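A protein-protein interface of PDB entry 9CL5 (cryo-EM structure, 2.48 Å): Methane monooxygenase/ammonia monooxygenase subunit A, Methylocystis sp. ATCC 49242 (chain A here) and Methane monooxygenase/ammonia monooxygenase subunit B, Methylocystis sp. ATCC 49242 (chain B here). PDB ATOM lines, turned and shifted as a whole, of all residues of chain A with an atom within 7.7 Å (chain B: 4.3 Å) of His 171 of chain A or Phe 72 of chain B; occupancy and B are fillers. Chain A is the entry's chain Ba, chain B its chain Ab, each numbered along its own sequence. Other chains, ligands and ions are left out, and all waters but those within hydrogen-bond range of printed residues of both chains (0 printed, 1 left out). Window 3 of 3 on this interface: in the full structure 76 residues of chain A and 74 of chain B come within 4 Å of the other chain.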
ATOM      1  N   THR A 168      17.439   6.716  -7.559  1.00  0.00           N
ATOM      2  CA  THR A 168      16.952   7.710  -6.618  1.00  0.00           C
ATOM      3  C   THR A 168      17.638   7.486  -5.277  1.00  0.00           C
ATOM      4  O   THR A 168      18.139   6.398  -4.988  1.00  0.00           O
ATOM      5  CB  THR A 168      15.424   7.643  -6.455  1.00  0.00           C
ATOM      6  OG1 THR A 168      14.993   8.641  -5.523  1.00  0.00           O
ATOM      7  CG2 THR A 168      14.996   6.273  -5.957  1.00  0.00           C
ATOM      8  N   GLU A 169      17.681   8.535  -4.462  1.00  0.00           N
ATOM      9  CA  GLU A 169      18.296   8.465  -3.143  1.00  0.00           C
ATOM     10  C   GLU A 169      17.229   8.681  -2.084  1.00  0.00           C
ATOM     11  O   GLU A 169      16.621   9.755  -2.017  1.00  0.00           O
ATOM     12  CB  GLU A 169      19.416   9.492  -2.989  1.00  0.00           C
ATOM     13  CG  GLU A 169      20.106   9.425  -1.638  1.00  0.00           C
ATOM     14  CD  GLU A 169      20.599  10.773  -1.168  1.00  0.00           C
ATOM     15  OE1 GLU A 169      20.603  11.721  -1.980  1.00  0.00           O
ATOM     16  OE2 GLU A 169      20.980  10.886   0.015  1.00  0.00           O
ATOM     17  N   GLN A 170      17.008   7.663  -1.262  1.00  0.00           N
ATOM     18  CA  GLN A 170      16.092   7.734  -0.141  1.00  0.00           C
ATOM     19  C   GLN A 170      16.844   8.192   1.104  1.00  0.00           C
ATOM     20  O   GLN A 170      17.922   8.784   1.023  1.00  0.00           O
ATOM     21  CB  GLN A 170      15.395   6.390   0.067  1.00  0.00           C
ATOM     22  CG  GLN A 170      14.632   5.937  -1.161  1.00  0.00           C
ATOM     23  CD  GLN A 170      13.580   6.944  -1.581  1.00  0.00           C
ATOM     24  OE1 GLN A 170      12.846   7.476  -0.749  1.00  0.00           O
ATOM     25  NE2 GLN A 170      13.514   7.226  -2.874  1.00  0.00           N
ATOM     26  N   HIS A 171      16.233   7.947   2.266  1.00  0.00           N
ATOM     27  CA  HIS A 171      16.752   8.430   3.544  1.00  0.00           C
ATOM     28  C   HIS A 171      18.266   8.287   3.669  1.00  0.00           C
ATOM     29  O   HIS A 171      18.965   9.253   3.986  1.00  0.00           O
ATOM     30  CB  HIS A 171      16.032   7.698   4.676  1.00  0.00           C
ATOM     31  CG  HIS A 171      14.565   7.984   4.725  1.00  0.00           C
ATOM     32  ND1 HIS A 171      13.664   7.393   3.866  1.00  0.00           N
ATOM     33  CD2 HIS A 171      13.842   8.814   5.514  1.00  0.00           C
ATOM     34  CE1 HIS A 171      12.451   7.844   4.125  1.00  0.00           C
ATOM     35  NE2 HIS A 171      12.531   8.706   5.123  1.00  0.00           N
ATOM     36  N   GLY A 172      18.791   7.091   3.423  1.00  0.00           N
ATOM     37  CA  GLY A 172      20.230   6.926   3.367  1.00  0.00           C
ATOM     38  C   GLY A 172      20.703   6.060   2.219  1.00  0.00           C
ATOM     39  O   GLY A 172      21.900   6.005   1.925  1.00  0.00           O
ATOM     40  N   GLN A 173      19.770   5.389   1.556  1.00  0.00           N
ATOM     41  CA  GLN A 173      20.077   4.323   0.613  1.00  0.00           C
ATOM     42  C   GLN A 173      19.871   4.784  -0.824  1.00  0.00           C
ATOM     43  O   GLN A 173      19.279   5.832  -1.098  1.00  0.00           O
ATOM     44  CB  GLN A 173      19.209   3.092   0.895  1.00  0.00           C
ATOM     45  CG  GLN A 173      19.504   2.407   2.211  1.00  0.00           C
ATOM     46  CD  GLN A 173      19.033   0.973   2.224  1.00  0.00           C
ATOM     47  OE1 GLN A 173      18.865   0.355   1.174  1.00  0.00           O
ATOM     48  NE2 GLN A 173      18.810   0.432   3.416  1.00  0.00           N
ATOM     49  N   LEU A 174      20.373   3.968  -1.743  1.00  0.00           N
ATOM     50  CA  LEU A 174      20.180   4.148  -3.173  1.00  0.00           C
ATOM     51  C   LEU A 174      19.176   3.115  -3.665  1.00  0.00           C
ATOM     52  O   LEU A 174      19.276   1.935  -3.317  1.00  0.00           O
ATOM     53  CB  LEU A 174      21.507   4.007  -3.923  1.00  0.00           C
ATOM     54  CG  LEU A 174      21.460   3.991  -5.450  1.00  0.00           C
ATOM     55  CD1 LEU A 174      21.304   5.397  -5.998  1.00  0.00           C
ATOM     56  CD2 LEU A 174      22.706   3.331  -6.006  1.00  0.00           C
ATOM     57  N   MET A 175      18.210   3.561  -4.466  1.00  0.00           N
ATOM     58  CA  MET A 175      17.126   2.717  -4.937  1.00  0.00           C
ATOM     59  C   MET A 175      16.968   2.873  -6.441  1.00  0.00           C
ATOM     60  O   MET A 175      17.379   3.873  -7.032  1.00  0.00           O
ATOM     61  CB  MET A 175      15.797   3.081  -4.265  1.00  0.00           C
ATOM     62  CG  MET A 175      15.663   2.678  -2.813  1.00  0.00           C
ATOM     63  SD  MET A 175      14.061   1.919  -2.500  1.00  0.00           S
ATOM     64  CE  MET A 175      13.853   2.302  -0.769  1.00  0.00           C
ATOM     65  N   PHE A 183       8.104  -1.029  -3.130  1.00  0.00           N
ATOM     66  CA  PHE A 183       8.074  -0.678  -1.714  1.00  0.00           C
ATOM     67  C   PHE A 183       6.860   0.180  -1.374  1.00  0.00           C
ATOM     68  O   PHE A 183       6.197  -0.053  -0.358  1.00  0.00           O
ATOM     69  CB  PHE A 183       9.371   0.041  -1.342  1.00  0.00           C
ATOM     70  CG  PHE A 183       9.513   0.339   0.123  1.00  0.00           C
ATOM     71  CD1 PHE A 183       9.679  -0.683   1.042  1.00  0.00           C
ATOM     72  CD2 PHE A 183       9.498   1.647   0.578  1.00  0.00           C
ATOM     73  CE1 PHE A 183       9.817  -0.407   2.386  1.00  0.00           C
ATOM     74  CE2 PHE A 183       9.634   1.927   1.922  1.00  0.00           C
ATOM     75  CZ  PHE A 183       9.795   0.899   2.826  1.00  0.00           C
ATOM     76  N   HIS A 184       6.553   1.171  -2.212  1.00  0.00           N
ATOM     77  CA  HIS A 184       5.487   2.119  -1.897  1.00  0.00           C
ATOM     78  C   HIS A 184       4.121   1.447  -1.922  1.00  0.00           C
ATOM     79  O   HIS A 184       3.320   1.609  -0.995  1.00  0.00           O
ATOM     80  CB  HIS A 184       5.524   3.293  -2.878  1.00  0.00           C
ATOM     81  CG  HIS A 184       6.465   4.385  -2.481  1.00  0.00           C
ATOM     82  ND1 HIS A 184       6.408   5.649  -3.024  1.00  0.00           N
ATOM     83  CD2 HIS A 184       7.490   4.402  -1.597  1.00  0.00           C
ATOM     84  CE1 HIS A 184       7.356   6.398  -2.490  1.00  0.00           C
ATOM     85  NE2 HIS A 184       8.026   5.665  -1.622  1.00  0.00           N
ATOM     86  N   LEU B  57       9.604  -6.351   7.662  1.00  0.00           N
ATOM     87  CA  LEU B  57       8.520  -5.604   8.285  1.00  0.00           C
ATOM     88  C   LEU B  57       7.527  -5.141   7.226  1.00  0.00           C
ATOM     89  O   LEU B  57       7.920  -4.686   6.149  1.00  0.00           O
ATOM     90  CB  LEU B  57       9.079  -4.404   9.050  1.00  0.00           C
ATOM     91  CG  LEU B  57       8.085  -3.405   9.640  1.00  0.00           C
ATOM     92  CD1 LEU B  57       7.466  -3.955  10.913  1.00  0.00           C
ATOM     93  CD2 LEU B  57       8.769  -2.075   9.904  1.00  0.00           C
ATOM     94  N   ALA B  70       7.937   5.163   3.862  1.00  0.00           N
ATOM     95  CA  ALA B  70       9.139   4.705   4.546  1.00  0.00           C
ATOM     96  C   ALA B  70       8.745   3.744   5.658  1.00  0.00           C
ATOM     97  O   ALA B  70       7.597   3.720   6.108  1.00  0.00           O
ATOM     98  CB  ALA B  70       9.943   5.878   5.114  1.00  0.00           C
ATOM     99  N   GLN B  71       9.720   2.953   6.093  1.00  0.00           N
ATOM    100  CA  GLN B  71       9.558   2.109   7.268  1.00  0.00           C
ATOM    101  C   GLN B  71      10.928   1.879   7.887  1.00  0.00           C
ATOM    102  O   GLN B  71      11.933   1.785   7.178  1.00  0.00           O
ATOM    103  CB  GLN B  71       8.878   0.774   6.932  1.00  0.00           C
ATOM    104  CG  GLN B  71       9.771  -0.258   6.274  1.00  0.00           C
ATOM    105  CD  GLN B  71       9.016  -1.497   5.852  1.00  0.00           C
ATOM    106  OE1 GLN B  71       7.801  -1.580   6.014  1.00  0.00           O
ATOM    107  NE2 GLN B  71       9.734  -2.473   5.313  1.00  0.00           N
ATOM    108  N   PHE B  72      10.956   1.810   9.215  1.00  0.00           N
ATOM    109  CA  PHE B  72      12.185   1.695   9.985  1.00  0.00           C
ATOM    110  C   PHE B  72      11.995   0.632  11.054  1.00  0.00           C
ATOM    111  O   PHE B  72      10.990   0.644  11.771  1.00  0.00           O
ATOM    112  CB  PHE B  72      12.561   3.033  10.637  1.00  0.00           C
ATOM    113  CG  PHE B  72      12.477   4.214   9.708  1.00  0.00           C
ATOM    114  CD1 PHE B  72      11.270   4.857   9.482  1.00  0.00           C
ATOM    115  CD2 PHE B  72      13.609   4.692   9.070  1.00  0.00           C
ATOM    116  CE1 PHE B  72      11.193   5.941   8.629  1.00  0.00           C
ATOM    117  CE2 PHE B  72      13.536   5.776   8.220  1.00  0.00           C
ATOM    118  CZ  PHE B  72      12.327   6.402   7.999  1.00  0.00           C
ATOM    119  N   ILE B  73      12.950  -0.289  11.160  1.00  0.00           N
ATOM    120  CA  ILE B  73      12.966  -1.274  12.235  1.00  0.00           C
ATOM    121  C   ILE B  73      14.398  -1.416  12.733  1.00  0.00           C
ATOM    122  O   ILE B  73      15.343  -1.448  11.939  1.00  0.00           O
ATOM    123  CB  ILE B  73      12.384  -2.635  11.790  1.00  0.00           C
ATOM    124  CG1 ILE B  73      12.306  -3.600  12.976  1.00  0.00           C
ATOM    125  CG2 ILE B  73      13.195  -3.243  10.654  1.00  0.00           C
ATOM    126  CD1 ILE B  73      11.038  -4.415  13.022  1.00  0.00           C
ATOM    127  N   GLN B  76      16.997   1.442  11.845  1.00  0.00           N
ATOM    128  CA  GLN B  76      17.501   1.415  10.481  1.00  0.00           C
ATOM    129  C   GLN B  76      16.343   1.527   9.502  1.00  0.00           C
ATOM    130  O   GLN B  76      15.296   0.904   9.701  1.00  0.00           O
ATOM    131  CB  GLN B  76      18.287   0.130  10.200  1.00  0.00           C
ATOM    132  CG  GLN B  76      19.704   0.130  10.736  1.00  0.00           C
ATOM    133  CD  GLN B  76      20.206  -1.265  11.044  1.00  0.00           C
ATOM    134  OE1 GLN B  76      20.046  -2.184  10.241  1.00  0.00           O
ATOM    135  NE2 GLN B  76      20.819  -1.428  12.209  1.00  0.00           N
ATOM    136  N   PHE B  77      16.537   2.316   8.450  1.00  0.00           N
ATOM    137  CA  PHE B  77      15.588   2.332   7.345  1.00  0.00           C
ATOM    138  C   PHE B  77      15.621   0.977   6.652  1.00  0.00           C
ATOM    139  O   PHE B  77      16.686   0.501   6.250  1.00  0.00           O
ATOM    140  CB  PHE B  77      15.935   3.453   6.366  1.00  0.00           C
ATOM    141  CG  PHE B  77      15.070   3.486   5.140  1.00  0.00           C
ATOM    142  CD1 PHE B  77      13.710   3.716   5.244  1.00  0.00           C
ATOM    143  CD2 PHE B  77      15.620   3.298   3.883  1.00  0.00           C
ATOM    144  CE1 PHE B  77      12.913   3.750   4.118  1.00  0.00           C
ATOM    145  CE2 PHE B  77      14.826   3.331   2.755  1.00  0.00           C
ATOM    146  CZ  PHE B  77      13.473   3.557   2.872  1.00  0.00           C
ATOM    147  N   ALA B  91      12.052  -1.779  18.035  1.00  0.00           N
ATOM    148  CA  ALA B  91      11.046  -0.764  17.759  1.00  0.00           C
ATOM    149  C   ALA B  91      10.904  -0.575  16.255  1.00  0.00           C
ATOM    150  O   ALA B  91      11.895  -0.611  15.520  1.00  0.00           O
ATOM    151  CB  ALA B  91      11.412   0.565  18.422  1.00  0.00           C
ATOM    152  N   PHE B  92       9.668  -0.383  15.798  1.00  0.00           N
ATOM    153  CA  PHE B  92       9.383  -0.217  14.381  1.00  0.00           C
ATOM    154  C   PHE B  92       8.427   0.947  14.166  1.00  0.00           C
ATOM    155  O   PHE B  92       7.635   1.297  15.045  1.00  0.00           O
ATOM    156  CB  PHE B  92       8.794  -1.502  13.763  1.00  0.00           C
ATOM    157  CG  PHE B  92       7.428  -1.863  14.282  1.00  0.00           C
ATOM    158  CD1 PHE B  92       6.284  -1.338  13.700  1.00  0.00           C
ATOM    159  CD2 PHE B  92       7.290  -2.735  15.348  1.00  0.00           C
ATOM    160  CE1 PHE B  92       5.036  -1.666  14.178  1.00  0.00           C
ATOM    161  CE2 PHE B  92       6.041  -3.069  15.826  1.00  0.00           C
ATOM    162  CZ  PHE B  92       4.914  -2.534  15.240  1.00  0.00           C
ATOM    163  N   SER B  93       8.517   1.531  12.974  1.00  0.00           N
ATOM    164  CA  SER B  93       7.674   2.643  12.559  1.00  0.00           C
ATOM    165  C   SER B  93       7.435   2.535  11.060  1.00  0.00           C
ATOM    166  O   SER B  93       8.328   2.126  10.317  1.00  0.00           O
ATOM    167  CB  SER B  93       8.321   3.988  12.903  1.00  0.00           C
ATOM    168  OG  SER B  93       7.580   5.065  12.362  1.00  0.00           O
ATOM    169  N   ASN B  95       5.490   4.777   7.798  1.00  0.00           N
ATOM    170  CA  ASN B  95       4.800   5.959   7.305  1.00  0.00           C
ATOM    171  C   ASN B  95       3.907   5.565   6.138  1.00  0.00           C
ATOM    172  O   ASN B  95       4.356   4.886   5.210  1.00  0.00           O
ATOM    173  CB  ASN B  95       5.800   7.030   6.865  1.00  0.00           C
ATOM    174  CG  ASN B  95       6.773   7.407   7.962  1.00  0.00           C
ATOM    175  OD1 ASN B  95       6.463   7.305   9.146  1.00  0.00           O
ATOM    176  ND2 ASN B  95       7.958   7.853   7.570  1.00  0.00           N
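O of Thr 168 of chain A sits at hydrogen-bond distance from N of Met 175 of chain A. The side-chain amide nitrogen of Gln 71 of chain B lies within hydrogen-bond range of the backbone carbonyl oxygen of Leu 57 of chain B (3.0 Å). The backbone carbonyl oxygen of Ala 70 of chain B is in hydrogen-bond range of the backbone NH of Asn 95 of chain B, 2.9 Å away. The backbone NH (N) of Phe 72 of chain B is in hydrogen-bond range of the backbone carbonyl oxygen (O) of Ser 93 of chain B, 2.9 Å away.
CE1 of His 171 of chain A touches CB of Ala 70 of chain B (3.3 Å). His 171 of chain A touches Phe 72 of chain B (NE2 to CZ, 3.7 Å). His 171 of chain A touches Phe 77 of chain B (ND1 to CE1, 3.7 Å). Gln 173 of chain A touches Phe 77 of chain B (NE2 to O, 3.5 Å). Phe 77 of chain B touches Met 175 of chain A. Phe 183 of chain A touches Ala 70 of chain B (CE2 to CA, 3.9 Å). Gln 71 of chain B touches Phe 183 of chain A (NE2 to CE1, 3.6 Å).
Thr 168 of chain A touches none of the printed residues of chain B. His 171 of chain A touches just these residues of chain B: Ala 70 (3.3 Å), Phe 72 (3.7 Å) and Phe 77 (3.7 Å). Gly 172 of chain A touches none of the printed residues of chain B. Printed residues of chain B within 4 Å of Met 175 of chain A: Phe 77 (3.8 Å). Printed residues of chain B within 4 Å of Phe 183 of chain A: Ala 70 and Gln 71. Of the printed residues of chain A, Ala 70 of chain B touches His 171 (3.3 Å) and Phe 183 (3.9 Å). Phe 72 of chain B touches one residue of chain A. Printed residues of chain A within 4 Å of Phe 77 of chain B: His 171, Gln 173 and Met 175. The nearest residue of chain A that does not touch Phe 72 of chain B is Phe 183 of chain A (6.6 Å). The nearest printed residue of chain A that does not touch Ala 70 of chain B is His 184 of chain A (5.5 Å).
Of the 11 printed residues of chain B, 4 touch a printed residue of chain A. Printed residues of chain B that touch a printed residue of chain A: Ala 70, Gln 71, Phe 72 and Phe 77. Hydrophobic or aromatic side chains of chain B that line the printed part of chain A: Ala 70, Phe 72 and Phe 77. Among the printed residues, 7 pairs touch across the chains.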
